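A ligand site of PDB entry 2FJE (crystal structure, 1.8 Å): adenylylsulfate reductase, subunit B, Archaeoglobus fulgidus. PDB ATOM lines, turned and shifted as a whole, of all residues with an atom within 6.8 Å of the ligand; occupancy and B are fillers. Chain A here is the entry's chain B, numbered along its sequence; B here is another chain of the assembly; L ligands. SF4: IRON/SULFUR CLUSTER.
The backbone NH (N) of Tyr 51 lies close to a sulfur (S1) of the ligand (3.4 Å). The side-chain amide nitrogen (ND2) of Asn 41 lies close to a sulfur (S3) of the ligand. FE2 of the ligand is bound by SG of Cys 47 (2.4 Å). A sulfur (S3) of the ligand sits close to the side-chain hydroxyl (OG) of Ser 3, 3.2 Å away. The backbone NH (N) of Trp 48 sits close to a sulfur (S4) of the ligand (3.6 Å). An iron atom (FE1) of the ligand is bound by the side-chain sulfur of Cys 25 (2.4 Å). The side-chain sulfur (SG) of Cys 50 is bound to an iron atom (FE3) of the ligand (2.4 Å). N of Cys 50 sits close to S1 of the ligand (3.4 Å). SG of Cys 53 binds FE4 of the ligand, 2.4 Å away. S2 of the ligand sits close to N of Cys 53 (3.4 Å).
The backbone NH (N) of Asp 28 sits close to the side-chain sulfur (SG) of Cys 25 (3.4 Å). OG of Ser 52 lies close to SG of Cys 50, 3.1 Å away. The side-chain sulfur (SG) of Cys 25 lies close to the backbone NH (N) of Leu 29 (3.2 Å). OG of Ser 3 is in hydrogen-bond range of SD of Met 30 (3.4 Å). SG of Cys 25 sits close to N of Asn 27 (3.4 Å). OE2 of Glu 49 sits close to N of Pro 2 (2.6 Å). ND2 of Asn 41 lies within hydrogen-bond range of OG of Ser 3 (3.1 Å). The side-chain sulfur of Cys 47 lies close to the backbone NH of Glu 49, 3.3 Å away.
The side-chain sulfur of Met 30 sits close to a sulfur (S3) of the ligand, 3.7 Å away. Residues that only touch the ligand: Pro 26, Leu 29, Glu 49 and Ser 52. Hydrophobic or aromatic side chains that line the ligand: Pro 26, Leu 29 and Met 30. Of the 27 residues printed, 13 come within 4 Å of the ligand.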
ATOM      1  N   PRO A   2     -15.169  17.837  13.743  1.00  0.00           N
ATOM      2  CA  PRO A   2     -16.130  18.930  13.556  1.00  0.00           C
ATOM      3  C   PRO A   2     -17.532  18.413  13.320  1.00  0.00           C
ATOM      4  O   PRO A   2     -17.729  17.231  13.014  1.00  0.00           O
ATOM      5  CB  PRO A   2     -15.571  19.657  12.332  1.00  0.00           C
ATOM      6  CG  PRO A   2     -14.092  19.446  12.471  1.00  0.00           C
ATOM      7  CD  PRO A   2     -13.997  17.993  12.862  1.00  0.00           C
ATOM      8  N   SER A   3     -18.522  19.287  13.449  1.00  0.00           N
ATOM      9  CA  SER A   3     -19.902  18.880  13.245  1.00  0.00           C
ATOM     10  C   SER A   3     -20.215  18.778  11.766  1.00  0.00           C
ATOM     11  O   SER A   3     -19.542  19.372  10.931  1.00  0.00           O
ATOM     12  CB  SER A   3     -20.857  19.902  13.881  1.00  0.00           C
ATOM     13  OG  SER A   3     -20.843  21.109  13.138  1.00  0.00           O
ATOM     14  N   PHE A   4     -21.241  18.001  11.438  1.00  0.00           N
ATOM     15  CA  PHE A   4     -21.691  17.859  10.067  1.00  0.00           C
ATOM     16  C   PHE A   4     -23.159  17.455  10.115  1.00  0.00           C
ATOM     17  O   PHE A   4     -23.600  16.743  11.023  1.00  0.00           O
ATOM     18  CB  PHE A   4     -20.846  16.828   9.294  1.00  0.00           C
ATOM     19  CG  PHE A   4     -21.095  15.398   9.678  1.00  0.00           C
ATOM     20  CD1 PHE A   4     -22.080  14.647   9.019  1.00  0.00           C
ATOM     21  CD2 PHE A   4     -20.343  14.785  10.670  1.00  0.00           C
ATOM     22  CE1 PHE A   4     -22.287  13.315   9.344  1.00  0.00           C
ATOM     23  CE2 PHE A   4     -20.552  13.448  11.012  1.00  0.00           C
ATOM     24  CZ  PHE A   4     -21.523  12.709  10.338  1.00  0.00           C
ATOM     25  N   CYS A  21     -29.466  24.941  15.136  1.00  0.00           N
ATOM     26  CA  CYS A  21     -28.006  24.884  15.033  1.00  0.00           C
ATOM     27  C   CYS A  21     -27.379  26.250  14.779  1.00  0.00           C
ATOM     28  O   CYS A  21     -26.377  26.612  15.417  1.00  0.00           O
ATOM     29  CB  CYS A  21     -27.595  23.899  13.922  1.00  0.00           C
ATOM     30  SG  CYS A  21     -28.195  24.309  12.263  1.00  0.00           S
ATOM     31  N   ILE A  24     -27.594  28.375  18.071  1.00  0.00           N
ATOM     32  CA  ILE A  24     -26.756  28.003  19.209  1.00  0.00           C
ATOM     33  C   ILE A  24     -25.228  28.043  19.078  1.00  0.00           C
ATOM     34  O   ILE A  24     -24.540  28.279  20.069  1.00  0.00           O
ATOM     35  CB  ILE A  24     -27.151  26.589  19.711  1.00  0.00           C
ATOM     36  CG1 ILE A  24     -26.761  26.422  21.190  1.00  0.00           C
ATOM     37  CG2 ILE A  24     -26.481  25.514  18.868  1.00  0.00           C
ATOM     38  CD1 ILE A  24     -27.621  27.230  22.135  1.00  0.00           C
ATOM     39  N   CYS A  25     -24.705  27.826  17.875  1.00  0.00           N
ATOM     40  CA  CYS A  25     -23.253  27.795  17.676  1.00  0.00           C
ATOM     41  C   CYS A  25     -22.475  28.991  18.217  1.00  0.00           C
ATOM     42  O   CYS A  25     -22.611  30.117  17.733  1.00  0.00           O
ATOM     43  CB  CYS A  25     -22.895  27.617  16.204  1.00  0.00           C
ATOM     44  SG  CYS A  25     -21.108  27.465  15.966  1.00  0.00           S
ATOM     45  N   PRO A  26     -21.626  28.756  19.231  1.00  0.00           N
ATOM     46  CA  PRO A  26     -20.806  29.797  19.859  1.00  0.00           C
ATOM     47  C   PRO A  26     -19.765  30.438  18.937  1.00  0.00           C
ATOM     48  O   PRO A  26     -19.241  31.509  19.248  1.00  0.00           O
ATOM     49  CB  PRO A  26     -20.153  29.072  21.040  1.00  0.00           C
ATOM     50  CG  PRO A  26     -21.110  27.940  21.323  1.00  0.00           C
ATOM     51  CD  PRO A  26     -21.457  27.474  19.939  1.00  0.00           C
ATOM     52  N   ASN A  27     -19.451  29.790  17.820  1.00  0.00           N
ATOM     53  CA  ASN A  27     -18.468  30.341  16.898  1.00  0.00           C
ATOM     54  C   ASN A  27     -19.057  30.721  15.538  1.00  0.00           C
ATOM     55  O   ASN A  27     -18.316  30.941  14.576  1.00  0.00           O
ATOM     56  CB  ASN A  27     -17.302  29.353  16.717  1.00  0.00           C
ATOM     57  CG  ASN A  27     -15.940  30.059  16.713  1.00  0.00           C
ATOM     58  OD1 ASN A  27     -15.816  31.217  17.102  1.00  0.00           O
ATOM     59  ND2 ASN A  27     -14.908  29.341  16.282  1.00  0.00           N
ATOM     60  N   ASP A  28     -20.373  30.795  15.455  1.00  0.00           N
ATOM     61  CA  ASP A  28     -21.080  31.181  14.224  1.00  0.00           C
ATOM     62  C   ASP A  28     -20.712  30.320  13.005  1.00  0.00           C
ATOM     63  O   ASP A  28     -20.497  30.835  11.910  1.00  0.00           O
ATOM     64  CB  ASP A  28     -20.809  32.656  13.920  1.00  0.00           C
ATOM     65  CG  ASP A  28     -21.637  33.181  12.760  1.00  0.00           C
ATOM     66  OD1 ASP A  28     -22.850  32.881  12.714  1.00  0.00           O
ATOM     67  OD2 ASP A  28     -21.101  33.911  11.902  1.00  0.00           O
ATOM     68  N   LEU A  29     -20.659  29.005  13.207  1.00  0.00           N
ATOM     69  CA  LEU A  29     -20.299  28.083  12.126  1.00  0.00           C
ATOM     70  C   LEU A  29     -21.487  27.471  11.397  1.00  0.00           C
ATOM     71  O   LEU A  29     -21.403  27.190  10.204  1.00  0.00           O
ATOM     72  CB  LEU A  29     -19.428  26.946  12.684  1.00  0.00           C
ATOM     73  CG  LEU A  29     -18.208  27.345  13.496  1.00  0.00           C
ATOM     74  CD1 LEU A  29     -17.413  26.080  13.844  1.00  0.00           C
ATOM     75  CD2 LEU A  29     -17.355  28.333  12.713  1.00  0.00           C
ATOM     76  N   MET A  30     -22.586  27.232  12.106  1.00  0.00           N
ATOM     77  CA  MET A  30     -23.758  26.620  11.486  1.00  0.00           C
ATOM     78  C   MET A  30     -24.605  27.646  10.744  1.00  0.00           C
ATOM     79  O   MET A  30     -24.937  28.709  11.283  1.00  0.00           O
ATOM     80  CB  MET A  30     -24.593  25.897  12.536  1.00  0.00           C
ATOM     81  CG  MET A  30     -23.850  24.785  13.287  1.00  0.00           C
ATOM     82  SD  MET A  30     -23.019  23.589  12.203  1.00  0.00           S
ATOM     83  CE  MET A  30     -24.441  22.776  11.440  1.00  0.00           C
ATOM     84  N   ASN A  41     -21.809  23.135   8.345  1.00  0.00           N
ATOM     85  CA  ASN A  41     -20.781  23.835   9.115  1.00  0.00           C
ATOM     86  C   ASN A  41     -19.974  24.595   8.061  1.00  0.00           C
ATOM     87  O   ASN A  41     -19.365  23.983   7.183  1.00  0.00           O
ATOM     88  CB  ASN A  41     -19.894  22.811   9.825  1.00  0.00           C
ATOM     89  CG  ASN A  41     -18.868  23.463  10.714  1.00  0.00           C
ATOM     90  OD1 ASN A  41     -18.222  24.442  10.324  1.00  0.00           O
ATOM     91  ND2 ASN A  41     -18.692  22.927  11.916  1.00  0.00           N
ATOM     92  N   PRO A  44     -15.350  24.346   9.349  1.00  0.00           N
ATOM     93  CA  PRO A  44     -14.991  23.253  10.240  1.00  0.00           C
ATOM     94  C   PRO A  44     -13.693  23.356  11.044  1.00  0.00           C
ATOM     95  O   PRO A  44     -13.618  22.808  12.144  1.00  0.00           O
ATOM     96  CB  PRO A  44     -15.024  22.028   9.325  1.00  0.00           C
ATOM     97  CG  PRO A  44     -14.668  22.591   7.990  1.00  0.00           C
ATOM     98  CD  PRO A  44     -15.475  23.870   7.964  1.00  0.00           C
ATOM     99  N   MET A  46     -12.714  25.697  12.645  1.00  0.00           N
ATOM    100  CA  MET A  46     -12.959  26.652  13.721  1.00  0.00           C
ATOM    101  C   MET A  46     -13.990  26.041  14.670  1.00  0.00           C
ATOM    102  O   MET A  46     -14.520  26.707  15.545  1.00  0.00           O
ATOM    103  CB  MET A  46     -13.469  27.986  13.171  1.00  0.00           C
ATOM    104  CG  MET A  46     -12.368  28.895  12.640  1.00  0.00           C
ATOM    105  SD  MET A  46     -11.265  29.476  13.960  1.00  0.00           S
ATOM    106  CE  MET A  46     -11.033  31.192  13.491  1.00  0.00           C
ATOM    107  N   CYS A  47     -14.262  24.739  14.474  1.00  0.00           N
ATOM    108  CA  CYS A  47     -15.204  24.009  15.302  1.00  0.00           C
ATOM    109  C   CYS A  47     -14.494  23.481  16.542  1.00  0.00           C
ATOM    110  O   CYS A  47     -13.474  22.792  16.437  1.00  0.00           O
ATOM    111  CB  CYS A  47     -15.818  22.845  14.520  1.00  0.00           C
ATOM    112  SG  CYS A  47     -16.997  21.806  15.465  1.00  0.00           S
ATOM    113  N   TRP A  48     -15.047  23.782  17.706  1.00  0.00           N
ATOM    114  CA  TRP A  48     -14.472  23.370  18.995  1.00  0.00           C
ATOM    115  C   TRP A  48     -15.002  22.001  19.402  1.00  0.00           C
ATOM    116  O   TRP A  48     -14.579  21.435  20.407  1.00  0.00           O
ATOM    117  CB  TRP A  48     -14.861  24.416  20.047  1.00  0.00           C
ATOM    118  CG  TRP A  48     -13.945  24.515  21.237  1.00  0.00           C
ATOM    119  CD1 TRP A  48     -12.582  24.611  21.209  1.00  0.00           C
ATOM    120  CD2 TRP A  48     -14.316  24.651  22.617  1.00  0.00           C
ATOM    121  NE1 TRP A  48     -12.078  24.804  22.478  1.00  0.00           N
ATOM    122  CE2 TRP A  48     -13.135  24.827  23.359  1.00  0.00           C
ATOM    123  CE3 TRP A  48     -15.551  24.637  23.292  1.00  0.00           C
ATOM    124  CZ2 TRP A  48     -13.137  24.998  24.746  1.00  0.00           C
ATOM    125  CZ3 TRP A  48     -15.549  24.804  24.672  1.00  0.00           C
ATOM    126  CH2 TRP A  48     -14.357  24.987  25.386  1.00  0.00           C
ATOM    127  N   GLU A  49     -15.911  21.462  18.591  1.00  0.00           N
ATOM    128  CA  GLU A  49     -16.565  20.177  18.865  1.00  0.00           C
ATOM    129  C   GLU A  49     -17.207  20.245  20.258  1.00  0.00           C
ATOM    130  O   GLU A  49     -17.019  19.349  21.086  1.00  0.00           O
ATOM    131  CB  GLU A  49     -15.575  19.007  18.775  1.00  0.00           C
ATOM    132  CG  GLU A  49     -15.099  18.702  17.352  1.00  0.00           C
ATOM    133  CD  GLU A  49     -14.448  17.323  17.192  1.00  0.00           C
ATOM    134  OE1 GLU A  49     -14.054  16.717  18.209  1.00  0.00           O
ATOM    135  OE2 GLU A  49     -14.315  16.863  16.038  1.00  0.00           O
ATOM    136  N   CYS A  50     -17.955  21.309  20.490  1.00  0.00           N
ATOM    137  CA  CYS A  50     -18.644  21.525  21.768  1.00  0.00           C
ATOM    138  C   CYS A  50     -19.975  20.780  21.837  1.00  0.00           C
ATOM    139  O   CYS A  50     -20.566  20.657  22.911  1.00  0.00           O
ATOM    140  CB  CYS A  50     -18.880  23.016  22.007  1.00  0.00           C
ATOM    141  SG  CYS A  50     -20.202  23.767  21.027  1.00  0.00           S
ATOM    142  N   TYR A  51     -20.424  20.293  20.684  1.00  0.00           N
ATOM    143  CA  TYR A  51     -21.678  19.532  20.575  1.00  0.00           C
ATOM    144  C   TYR A  51     -22.953  20.311  20.869  1.00  0.00           C
ATOM    145  O   TYR A  51     -24.019  19.724  21.052  1.00  0.00           O
ATOM    146  CB  TYR A  51     -21.628  18.292  21.471  1.00  0.00           C
ATOM    147  CG  TYR A  51     -20.845  17.128  20.883  1.00  0.00           C
ATOM    148  CD1 TYR A  51     -19.463  17.181  20.773  1.00  0.00           C
ATOM    149  CD2 TYR A  51     -21.507  15.986  20.421  1.00  0.00           C
ATOM    150  CE1 TYR A  51     -18.740  16.110  20.218  1.00  0.00           C
ATOM    151  CE2 TYR A  51     -20.792  14.916  19.860  1.00  0.00           C
ATOM    152  CZ  TYR A  51     -19.415  14.988  19.761  1.00  0.00           C
ATOM    153  OH  TYR A  51     -18.718  13.925  19.224  1.00  0.00           O
ATOM    154  N   SER A  52     -22.879  21.639  20.897  1.00  0.00           N
ATOM    155  CA  SER A  52     -24.065  22.447  21.171  1.00  0.00           C
ATOM    156  C   SER A  52     -25.088  22.235  20.067  1.00  0.00           C
ATOM    157  O   SER A  52     -26.256  21.966  20.341  1.00  0.00           O
ATOM    158  CB  SER A  52     -23.704  23.920  21.283  1.00  0.00           C
ATOM    159  OG  SER A  52     -22.963  24.171  22.468  1.00  0.00           O
ATOM    160  N   CYS A  53     -24.642  22.365  18.820  1.00  0.00           N
ATOM    161  CA  CYS A  53     -25.539  22.179  17.680  1.00  0.00           C
ATOM    162  C   CYS A  53     -26.148  20.787  17.683  1.00  0.00           C
ATOM    163  O   CYS A  53     -27.350  20.615  17.464  1.00  0.00           O
ATOM    164  CB  CYS A  53     -24.779  22.415  16.364  1.00  0.00           C
ATOM    165  SG  CYS A  53     -23.325  21.356  16.117  1.00  0.00           S
ATOM    166  N   VAL A  54     -25.311  19.770  17.928  1.00  0.00           N
ATOM    167  CA  VAL A  54     -25.780  18.392  17.971  1.00  0.00           C
ATOM    168  C   VAL A  54     -26.924  18.215  18.958  1.00  0.00           C
ATOM    169  O   VAL A  54     -27.954  17.622  18.632  1.00  0.00           O
ATOM    170  CB  VAL A  54     -24.641  17.435  18.374  1.00  0.00           C
ATOM    171  CG1 VAL A  54     -25.177  16.013  18.519  1.00  0.00           C
ATOM    172  CG2 VAL A  54     -23.533  17.479  17.336  1.00  0.00           C
ATOM    173  N   ILE A  62     -27.565  16.232  13.327  1.00  0.00           N
ATOM    174  CA  ILE A  62     -26.176  16.667  13.431  1.00  0.00           C
ATOM    175  C   ILE A  62     -25.339  15.687  14.245  1.00  0.00           C
ATOM    176  O   ILE A  62     -25.763  15.197  15.281  1.00  0.00           O
ATOM    177  CB  ILE A  62     -26.073  18.066  14.064  1.00  0.00           C
ATOM    178  CG1 ILE A  62     -27.003  19.044  13.331  1.00  0.00           C
ATOM    179  CG2 ILE A  62     -24.630  18.576  13.977  1.00  0.00           C
ATOM    180  CD1 ILE A  62     -26.939  20.461  13.840  1.00  0.00           C
ATOM    181  N   VAL A  64     -20.859  14.514  14.955  1.00  0.00           N
ATOM    182  CA  VAL A  64     -19.499  15.044  14.925  1.00  0.00           C
ATOM    183  C   VAL A  64     -18.549  13.965  14.443  1.00  0.00           C
ATOM    184  O   VAL A  64     -18.611  12.822  14.892  1.00  0.00           O
ATOM    185  CB  VAL A  64     -19.055  15.537  16.326  1.00  0.00           C
ATOM    186  CG1 VAL A  64     -17.570  15.851  16.315  1.00  0.00           C
ATOM    187  CG2 VAL A  64     -19.848  16.779  16.705  1.00  0.00           C
ATOM    188  N   ALA B  67     -19.467  26.296  26.948  1.00  0.00           N
ATOM    189  CA  ALA B  67     -20.396  25.787  25.945  1.00  0.00           C
ATOM    190  C   ALA B  67     -20.723  24.302  26.091  1.00  0.00           C
ATOM    191  O   ALA B  67     -21.875  23.898  25.896  1.00  0.00           O
ATOM    192  CB  ALA B  67     -19.851  26.055  24.546  1.00  0.00           C
ATOM    193  N   ILE B 237     -12.048  28.592  22.031  1.00  0.00           N
ATOM    194  CA  ILE B 237     -11.686  29.107  20.708  1.00  0.00           C
ATOM    195  C   ILE B 237     -12.553  30.326  20.390  1.00  0.00           C
ATOM    196  O   ILE B 237     -12.207  31.150  19.547  1.00  0.00           O
ATOM    197  CB  ILE B 237     -11.896  28.019  19.628  1.00  0.00           C
ATOM    198  CG1 ILE B 237     -11.323  28.477  18.290  1.00  0.00           C
ATOM    199  CG2 ILE B 237     -13.385  27.699  19.499  1.00  0.00           C
ATOM    200  CD1 ILE B 237     -11.274  27.386  17.243  1.00  0.00           C
ATOM    201  N   PHE B 238     -13.665  30.457  21.109  1.00  0.00           N
ATOM    202  CA  PHE B 238     -14.601  31.550  20.924  1.00  0.00           C
ATOM    203  C   PHE B 238     -14.076  32.890  21.458  1.00  0.00           C
ATOM    204  O   PHE B 238     -14.583  33.946  21.091  1.00  0.00           O
ATOM    205  CB  PHE B 238     -15.922  31.247  21.632  1.00  0.00           C
ATOM    206  CG  PHE B 238     -16.361  29.812  21.511  1.00  0.00           C
ATOM    207  CD1 PHE B 238     -16.568  29.043  22.646  1.00  0.00           C
ATOM    208  CD2 PHE B 238     -16.564  29.239  20.260  1.00  0.00           C
ATOM    209  CE1 PHE B 238     -16.968  27.718  22.553  1.00  0.00           C
ATOM    210  CE2 PHE B 238     -16.962  27.905  20.147  1.00  0.00           C
ATOM    211  CZ  PHE B 238     -17.171  27.146  21.302  1.00  0.00           C
HETATM  212 FE1  SF4 L   1     -20.484  25.245  16.606  1.00  0.00          FE
HETATM  213 FE2  SF4 L   1     -18.812  23.113  16.277  1.00  0.00          FE
HETATM  214 FE3  SF4 L   1     -19.986  23.641  18.656  1.00  0.00          FE
HETATM  215 FE4  SF4 L   1     -21.464  22.775  16.605  1.00  0.00          FE
HETATM  216  S1  SF4 L   1     -19.800  21.581  17.650  1.00  0.00           S
HETATM  217  S2  SF4 L   1     -21.995  24.328  18.018  1.00  0.00           S
HETATM  218  S3  SF4 L   1     -20.415  23.729  14.856  1.00  0.00           S
HETATM  219  S4  SF4 L   1     -18.438  24.904  17.619  1.00  0.00           S
